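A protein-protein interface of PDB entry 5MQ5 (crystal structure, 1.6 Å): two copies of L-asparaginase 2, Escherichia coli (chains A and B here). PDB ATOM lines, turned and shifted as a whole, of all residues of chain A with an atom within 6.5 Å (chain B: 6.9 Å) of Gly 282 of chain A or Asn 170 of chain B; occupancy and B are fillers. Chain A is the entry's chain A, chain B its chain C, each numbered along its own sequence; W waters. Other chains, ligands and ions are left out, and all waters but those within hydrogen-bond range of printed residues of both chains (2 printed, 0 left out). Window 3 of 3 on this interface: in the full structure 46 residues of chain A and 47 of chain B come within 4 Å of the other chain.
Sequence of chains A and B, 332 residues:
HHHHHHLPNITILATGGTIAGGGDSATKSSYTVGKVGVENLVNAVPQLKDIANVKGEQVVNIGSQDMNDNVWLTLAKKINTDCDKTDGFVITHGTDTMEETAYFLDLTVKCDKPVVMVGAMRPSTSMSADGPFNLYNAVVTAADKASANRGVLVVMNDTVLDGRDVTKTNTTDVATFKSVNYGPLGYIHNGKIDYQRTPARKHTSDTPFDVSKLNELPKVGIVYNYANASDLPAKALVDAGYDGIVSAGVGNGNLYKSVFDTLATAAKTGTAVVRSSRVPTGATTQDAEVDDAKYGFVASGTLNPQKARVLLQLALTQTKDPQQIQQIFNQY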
ATOM      1  N   VAL A 180      10.335  -0.034 -12.951  1.00  0.00           N
ATOM      2  CA  VAL A 180       9.975   1.377 -12.819  1.00  0.00           C
ATOM      3  C   VAL A 180       8.950   1.865 -13.839  1.00  0.00           C
ATOM      4  O   VAL A 180       8.391   2.961 -13.661  1.00  0.00           O
ATOM      5  CB  VAL A 180      11.235   2.258 -12.912  1.00  0.00           C
ATOM      6  CG1 VAL A 180      12.161   1.955 -11.753  1.00  0.00           C
ATOM      7  CG2 VAL A 180      11.977   2.044 -14.247  1.00  0.00           C
ATOM      8  N   ASN A 181       8.701   1.101 -14.905  1.00  0.00           N
ATOM      9  CA  ASN A 181       7.735   1.506 -15.913  1.00  0.00           C
ATOM     10  C   ASN A 181       6.412   0.765 -15.799  1.00  0.00           C
ATOM     11  O   ASN A 181       5.356   1.387 -15.961  1.00  0.00           O
ATOM     12  CB  ASN A 181       8.309   1.278 -17.308  1.00  0.00           C
ATOM     13  CG  ASN A 181       9.520   2.123 -17.570  1.00  0.00           C
ATOM     14  OD1 ASN A 181       9.422   3.349 -17.628  1.00  0.00           O
ATOM     15  ND2 ASN A 181      10.688   1.477 -17.689  1.00  0.00           N
ATOM     16  N   GLY A 251      16.917  13.218 -22.461  1.00  0.00           N
ATOM     17  CA  GLY A 251      15.480  13.260 -22.686  1.00  0.00           C
ATOM     18  C   GLY A 251      14.985  12.052 -23.455  1.00  0.00           C
ATOM     19  O   GLY A 251      15.342  10.904 -23.159  1.00  0.00           O
ATOM     20  N   ASN A 252      14.163  12.313 -24.474  1.00  0.00           N
ATOM     21  CA  ASN A 252      13.569  11.254 -25.300  1.00  0.00           C
ATOM     22  C   ASN A 252      14.567  10.826 -26.382  1.00  0.00           C
ATOM     23  O   ASN A 252      14.370  11.028 -27.583  1.00  0.00           O
ATOM     24  CB  ASN A 252      12.251  11.750 -25.887  1.00  0.00           C
ATOM     25  CG  ASN A 252      11.427  10.652 -26.541  1.00  0.00           C
ATOM     26  OD1 ASN A 252      11.886   9.528 -26.721  1.00  0.00           O
ATOM     27  ND2 ASN A 252      10.189  10.989 -26.899  1.00  0.00           N
ATOM     28  N   SER A 277      18.032   6.156 -23.534  1.00  0.00           N
ATOM     29  CA  SER A 277      18.071   7.402 -22.784  1.00  0.00           C
ATOM     30  C   SER A 277      18.705   7.204 -21.419  1.00  0.00           C
ATOM     31  O   SER A 277      18.450   6.201 -20.751  1.00  0.00           O
ATOM     32  CB  SER A 277      16.660   7.975 -22.589  1.00  0.00           C
ATOM     33  OG  SER A 277      16.723   9.161 -21.811  1.00  0.00           O
ATOM     34  N   VAL A 279      17.723   8.957 -19.079  1.00  0.00           N
ATOM     35  CA  VAL A 279      16.591   9.240 -18.194  1.00  0.00           C
ATOM     36  C   VAL A 279      16.061   7.920 -17.633  1.00  0.00           C
ATOM     37  O   VAL A 279      15.865   6.955 -18.400  1.00  0.00           O
ATOM     38  CB  VAL A 279      15.514  10.011 -18.960  1.00  0.00           C
ATOM     39  CG1 VAL A 279      14.344  10.322 -18.073  1.00  0.00           C
ATOM     40  CG2 VAL A 279      16.098  11.340 -19.474  1.00  0.00           C
ATOM     41  N   PRO A 280      15.826   7.818 -16.321  1.00  0.00           N
ATOM     42  CA  PRO A 280      15.663   6.485 -15.703  1.00  0.00           C
ATOM     43  C   PRO A 280      14.317   5.823 -15.909  1.00  0.00           C
ATOM     44  O   PRO A 280      14.208   4.620 -15.631  1.00  0.00           O
ATOM     45  CB  PRO A 280      15.893   6.753 -14.209  1.00  0.00           C
ATOM     46  CG  PRO A 280      15.587   8.247 -14.018  1.00  0.00           C
ATOM     47  CD  PRO A 280      16.031   8.884 -15.319  1.00  0.00           C
ATOM     48  N   THR A 281      13.282   6.549 -16.327  1.00  0.00           N
ATOM     49  CA  THR A 281      11.995   5.923 -16.622  1.00  0.00           C
ATOM     50  C   THR A 281      11.449   6.487 -17.920  1.00  0.00           C
ATOM     51  O   THR A 281      11.834   7.572 -18.362  1.00  0.00           O
ATOM     52  CB  THR A 281      10.959   6.131 -15.498  1.00  0.00           C
ATOM     53  OG1 THR A 281      10.516   7.495 -15.480  1.00  0.00           O
ATOM     54  CG2 THR A 281      11.548   5.785 -14.118  1.00  0.00           C
ATOM     55  N   GLY A 282      10.556   5.726 -18.545  1.00  0.00           N
ATOM     56  CA  GLY A 282       9.920   6.201 -19.754  1.00  0.00           C
ATOM     57  C   GLY A 282      10.586   5.648 -21.001  1.00  0.00           C
ATOM     58  O   GLY A 282      11.752   5.248 -21.002  1.00  0.00           O
ATOM     59  N   ALA A 283       9.821   5.635 -22.088  1.00  0.00           N
ATOM     60  CA  ALA A 283      10.319   5.101 -23.348  1.00  0.00           C
ATOM     61  C   ALA A 283      11.095   6.142 -24.144  1.00  0.00           C
ATOM     62  O   ALA A 283      10.763   7.334 -24.148  1.00  0.00           O
ATOM     63  CB  ALA A 283       9.158   4.606 -24.206  1.00  0.00           C
ATOM     64  N   THR A 284      12.104   5.661 -24.873  1.00  0.00           N
ATOM     65  CA  THR A 284      12.632   6.390 -26.021  1.00  0.00           C
ATOM     66  C   THR A 284      11.764   5.998 -27.211  1.00  0.00           C
ATOM     67  O   THR A 284      11.787   4.844 -27.656  1.00  0.00           O
ATOM     68  CB  THR A 284      14.103   6.072 -26.268  1.00  0.00           C
ATOM     69  OG1 THR A 284      14.889   6.558 -25.166  1.00  0.00           O
ATOM     70  CG2 THR A 284      14.584   6.768 -27.552  1.00  0.00           C
ATOM     71  N   GLY A 301      12.577   2.158 -26.922  1.00  0.00           N
ATOM     72  CA  GLY A 301      11.416   2.002 -26.048  1.00  0.00           C
ATOM     73  C   GLY A 301      11.815   2.156 -24.596  1.00  0.00           C
ATOM     74  O   GLY A 301      12.656   2.991 -24.250  1.00  0.00           O
ATOM     75  N   THR A 302      11.227   1.339 -23.724  1.00  0.00           N
ATOM     76  CA  THR A 302      11.524   1.502 -22.306  1.00  0.00           C
ATOM     77  C   THR A 302      12.836   0.847 -21.900  1.00  0.00           C
ATOM     78  O   THR A 302      13.204   0.926 -20.725  1.00  0.00           O
ATOM     79  CB  THR A 302      10.382   0.958 -21.416  1.00  0.00           C
ATOM     80  OG1 THR A 302      10.201  -0.451 -21.622  1.00  0.00           O
ATOM     81  CG2 THR A 302       9.070   1.706 -21.670  1.00  0.00           C
ATOM     82  N   LEU A 303      13.551   0.214 -22.823  1.00  0.00           N
ATOM     83  CA  LEU A 303      14.832  -0.392 -22.477  1.00  0.00           C
ATOM     84  C   LEU A 303      15.858   0.696 -22.198  1.00  0.00           C
ATOM     85  O   LEU A 303      16.130   1.530 -23.069  1.00  0.00           O
ATOM     86  CB  LEU A 303      15.307  -1.287 -23.611  1.00  0.00           C
ATOM     87  CG  LEU A 303      14.371  -2.466 -23.910  1.00  0.00           C
ATOM     88  CD1 LEU A 303      14.858  -3.177 -25.161  1.00  0.00           C
ATOM     89  CD2 LEU A 303      14.308  -3.427 -22.734  1.00  0.00           C
ATOM     90  N   MET B 121       7.467  20.096 -21.592  1.00  0.00           N
ATOM     91  CA  MET B 121       7.617  18.758 -22.156  1.00  0.00           C
ATOM     92  C   MET B 121       6.800  18.573 -23.427  1.00  0.00           C
ATOM     93  O   MET B 121       7.109  17.679 -24.230  1.00  0.00           O
ATOM     94  CB  MET B 121       7.236  17.711 -21.106  1.00  0.00           C
ATOM     95  CG  MET B 121       8.237  17.617 -19.970  1.00  0.00           C
ATOM     96  SD  MET B 121       9.804  16.937 -20.541  1.00  0.00           S
ATOM     97  CE  MET B 121       9.338  15.195 -20.620  1.00  0.00           C
ATOM     98  N   THR B 167      16.384  16.666 -11.355  1.00  0.00           N
ATOM     99  CA  THR B 167      16.775  15.847 -12.504  1.00  0.00           C
ATOM    100  C   THR B 167      15.528  15.449 -13.280  1.00  0.00           C
ATOM    101  O   THR B 167      14.423  15.431 -12.744  1.00  0.00           O
ATOM    102  CB  THR B 167      17.585  14.618 -12.046  1.00  0.00           C
ATOM    103  OG1 THR B 167      18.060  13.866 -13.180  1.00  0.00           O
ATOM    104  CG2 THR B 167      16.751  13.703 -11.139  1.00  0.00           C
ATOM    105  N   LYS B 168      15.714  15.121 -14.564  1.00  0.00           N
ATOM    106  CA  LYS B 168      14.622  14.692 -15.432  1.00  0.00           C
ATOM    107  C   LYS B 168      14.440  13.187 -15.248  1.00  0.00           C
ATOM    108  O   LYS B 168      15.339  12.409 -15.576  1.00  0.00           O
ATOM    109  CB  LYS B 168      14.930  15.055 -16.886  1.00  0.00           C
ATOM    110  CG  LYS B 168      13.841  14.692 -17.885  1.00  0.00           C
ATOM    111  CD  LYS B 168      14.157  15.318 -19.257  1.00  0.00           C
ATOM    112  CE  LYS B 168      13.020  15.101 -20.229  1.00  0.00           C
ATOM    113  NZ  LYS B 168      13.283  15.827 -21.511  1.00  0.00           N
ATOM    114  N   THR B 169      13.310  12.775 -14.663  1.00  0.00           N
ATOM    115  CA  THR B 169      13.149  11.370 -14.290  1.00  0.00           C
ATOM    116  C   THR B 169      12.434  10.533 -15.337  1.00  0.00           C
ATOM    117  O   THR B 169      12.525   9.298 -15.275  1.00  0.00           O
ATOM    118  CB  THR B 169      12.382  11.222 -12.965  1.00  0.00           C
ATOM    119  OG1 THR B 169      11.013  11.644 -13.100  1.00  0.00           O
ATOM    120  CG2 THR B 169      13.071  11.975 -11.858  1.00  0.00           C
ATOM    121  N   ASN B 170      11.722  11.161 -16.273  1.00  0.00           N
ATOM    122  CA  ASN B 170      10.917  10.437 -17.253  1.00  0.00           C
ATOM    123  C   ASN B 170      11.068  11.094 -18.620  1.00  0.00           C
ATOM    124  O   ASN B 170      11.178  12.313 -18.734  1.00  0.00           O
ATOM    125  CB  ASN B 170       9.430  10.398 -16.832  1.00  0.00           C
ATOM    126  CG  ASN B 170       8.578   9.554 -17.764  1.00  0.00           C
ATOM    127  OD1 ASN B 170       8.041  10.053 -18.753  1.00  0.00           O
ATOM    128  ND2 ASN B 170       8.457   8.260 -17.459  1.00  0.00           N
ATOM    129  N   THR B 171      11.021  10.275 -19.672  1.00  0.00           N
ATOM    130  CA  THR B 171      11.321  10.792 -21.006  1.00  0.00           C
ATOM    131  C   THR B 171      10.199  11.663 -21.570  1.00  0.00           C
ATOM    132  O   THR B 171      10.465  12.506 -22.440  1.00  0.00           O
ATOM    133  CB  THR B 171      11.551   9.633 -21.976  1.00  0.00           C
ATOM    134  OG1 THR B 171      10.414   8.764 -21.884  1.00  0.00           O
ATOM    135  CG2 THR B 171      12.823   8.861 -21.637  1.00  0.00           C
ATOM    136  N   THR B 172       8.946  11.471 -21.126  1.00  0.00           N
ATOM    137  CA  THR B 172       7.810  12.159 -21.752  1.00  0.00           C
ATOM    138  C   THR B 172       6.848  12.849 -20.788  1.00  0.00           C
ATOM    139  O   THR B 172       6.116  13.742 -21.226  1.00  0.00           O
ATOM    140  CB  THR B 172       7.005  11.176 -22.619  1.00  0.00           C
ATOM    141  OG1 THR B 172       6.582  10.076 -21.810  1.00  0.00           O
ATOM    142  CG2 THR B 172       7.875  10.632 -23.773  1.00  0.00           C
ATOM    143  N   ASP B 173       6.830  12.480 -19.510  1.00  0.00           N
ATOM    144  CA  ASP B 173       5.834  12.946 -18.552  1.00  0.00           C
ATOM    145  C   ASP B 173       6.010  14.433 -18.250  1.00  0.00           C
ATOM    146  O   ASP B 173       7.123  14.892 -17.974  1.00  0.00           O
ATOM    147  CB  ASP B 173       6.004  12.117 -17.279  1.00  0.00           C
ATOM    148  CG  ASP B 173       4.865  12.253 -16.277  1.00  0.00           C
ATOM    149  OD1 ASP B 173       4.088  13.238 -16.273  1.00  0.00           O
ATOM    150  OD2 ASP B 173       4.790  11.323 -15.442  1.00  0.00           O
ATOM    151  N   VAL B 174       4.906  15.190 -18.273  1.00  0.00           N
ATOM    152  CA  VAL B 174       4.969  16.586 -17.841  1.00  0.00           C
ATOM    153  C   VAL B 174       5.462  16.717 -16.407  1.00  0.00           C
ATOM    154  O   VAL B 174       6.006  17.769 -16.039  1.00  0.00           O
ATOM    155  CB  VAL B 174       3.606  17.296 -18.004  1.00  0.00           C
ATOM    156  CG1 VAL B 174       3.243  17.392 -19.479  1.00  0.00           C
ATOM    157  CG2 VAL B 174       2.494  16.612 -17.156  1.00  0.00           C
ATOM    158  N   ALA B 175       5.307  15.675 -15.585  1.00  0.00           N
ATOM    159  CA  ALA B 175       5.746  15.709 -14.193  1.00  0.00           C
ATOM    160  C   ALA B 175       7.167  15.191 -14.010  1.00  0.00           C
ATOM    161  O   ALA B 175       7.555  14.864 -12.882  1.00  0.00           O
ATOM    162  CB  ALA B 175       4.786  14.890 -13.324  1.00  0.00           C
ATOM    163  N   THR B 176       7.951  15.155 -15.091  1.00  0.00           N
ATOM    164  CA  THR B 176       9.246  14.487 -15.099  1.00  0.00           C
ATOM    165  C   THR B 176      10.253  15.055 -14.086  1.00  0.00           C
ATOM    166  O   THR B 176      11.078  14.295 -13.560  1.00  0.00           O
ATOM    167  CB  THR B 176       9.827  14.547 -16.516  1.00  0.00           C
ATOM    168  OG1 THR B 176      11.094  13.884 -16.526  1.00  0.00           O
ATOM    169  CG2 THR B 176      10.000  15.996 -16.985  1.00  0.00           C
ATOM    170  N   PHE B 177      10.241  16.364 -13.803  1.00  0.00           N
ATOM    171  CA  PHE B 177      11.325  16.925 -12.996  1.00  0.00           C
ATOM    172  C   PHE B 177      11.077  16.703 -11.506  1.00  0.00           C
ATOM    173  O   PHE B 177      10.064  17.155 -10.950  1.00  0.00           O
ATOM    174  CB  PHE B 177      11.530  18.405 -13.309  1.00  0.00           C
ATOM    175  CG  PHE B 177      12.307  18.623 -14.569  1.00  0.00           C
ATOM    176  CD1 PHE B 177      13.687  18.489 -14.581  1.00  0.00           C
ATOM    177  CD2 PHE B 177      11.644  18.879 -15.762  1.00  0.00           C
ATOM    178  CE1 PHE B 177      14.409  18.644 -15.765  1.00  0.00           C
ATOM    179  CE2 PHE B 177      12.348  19.049 -16.947  1.00  0.00           C
ATOM    180  CZ  PHE B 177      13.734  18.921 -16.953  1.00  0.00           C
HETATM  181  O   HOH W   1       7.482   7.470 -21.865  1.00  0.00           O
HETATM  182  O   HOH W   2       7.528   5.228 -17.125  1.00  0.00           O
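Of the 14 printed residues of chain A, 8 touch a printed residue of chain B.
Hydrophobic or aromatic side chains of chain A within 4 Å of the printed part of chain B: Val 279 and Pro 280.
Among the printed residues, no Asp or Glu carboxylate lies within 4 Å of a Lys or Arg side-chain nitrogen of the other chain.
The side-chain hydroxyl (OG1) of Thr 281 of chain A sits at hydrogen-bond distance from the backbone carbonyl oxygen (O) of Thr 169 of chain B (2.7 Å).
OG1 of Thr 281 of chain A lies within hydrogen-bond range of ND2 of Asn 170 of chain B, 3.0 Å away.
The backbone carbonyl oxygen (O) of Thr 281 of chain A lies within hydrogen-bond range of the backbone NH (N) of Thr 171 of chain B, at 3.1 Å.
N of Gly 282 of chain A sits close to ND2 of Asn 170 of chain B (3.5 Å).
The backbone carbonyl oxygen (O) of Ala 283 of chain A is in hydrogen-bond range of the side-chain hydroxyl (OG1) of Thr 171 of chain B, 2.7 Å away.
Printed residues of chain B within 4 Å of Gly 251 of chain A: Lys 168 (3.6 Å) and Thr 171 (3.6 Å).
Of the printed residues of chain B, Val 279 of chain A touches Lys 168, Thr 169, Asn 170 and Thr 171.
Of the printed residues of chain B, Pro 280 of chain A touches Lys 168 and Thr 169.
Printed residues of chain B within 4 Å of Thr 281 of chain A: Thr 169, Asn 170 and Thr 171.
Gly 282 of chain A touches just these residues of chain B: Asn 170 (3.4 Å) and Thr 171 (3.2 Å).
Printed residues of chain B within 4 Å of Ala 283 of chain A: Thr 171 (2.7 Å).
Of the printed residues of chain A, Asn 170 of chain B touches Val 279, Thr 281 and Gly 282.
The nearest residue of chain B that does not touch Gly 282 of chain A is Thr 169 of chain B (5.2 Å).
The nearest residue of chain A that does not touch Asn 170 of chain B is Pro 280 of chain A (5.0 Å).
The side-chain amide oxygen of Asn 181 of chain A is in hydrogen-bond range of the backbone NH of Gly 282 of chain A (2.8 Å).
O of Gly 251 of chain A lies within hydrogen-bond range of OG of Ser 277 of chain A (2.6 Å).
The side-chain hydroxyl of Ser 277 of chain A sits at hydrogen-bond distance from the backbone NH of Val 279 of chain A (2.9 Å).
SD of Met 121 of chain B lies close to NZ of Lys 168 of chain B.
N of Thr 172 of chain B sits at hydrogen-bond distance from OD1 of Asn 170 of chain B (2.9 Å).
N of Asp 173 of chain B sits at hydrogen-bond distance from OD1 of Asn 170 of chain B (2.8 Å).
No position is printed for both chains.
CA of Gly 251 of chain A touches NZ of Lys 168 of chain B, at 3.6 Å.
Gly 251 of chain A touches Thr 171 of chain B.
Asn 252 of chain A touches Thr 171 of chain B.
Ser 277 of chain A touches Thr 171 of chain B.
Val 279 of chain A touches Lys 168 of chain B (CG1 to O, 3.4 Å).
Val 279 of chain A touches Thr 169 of chain B.
N of Asn 170 of chain B touches CG1 of Val 279 of chain A, 3.3 Å away.
Val 279 of chain A touches Thr 171 of chain B.
O of Thr 169 of chain B touches CG of Pro 280 of chain A, at 3.5 Å.
Gly 282 of chain A touches Thr 171 of chain B (C to OG1, 3.2 Å).
Water W2 lies within hydrogen-bond range of the side-chain amide oxygen (OD1) of Asn 181 of chain A (2.7 Å), the side-chain amide nitrogen (ND2) of Asn 170 of chain B (3.2 Å) and the backbone NH (N) of Gly 282 of chain A (3.4 Å).
Water W1 lies within hydrogen-bond range of OG1 of Thr 172 of chain B (2.8 Å), N of Ala 283 of chain A (3.0 Å) and OG1 of Thr 171 of chain B (3.2 Å).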
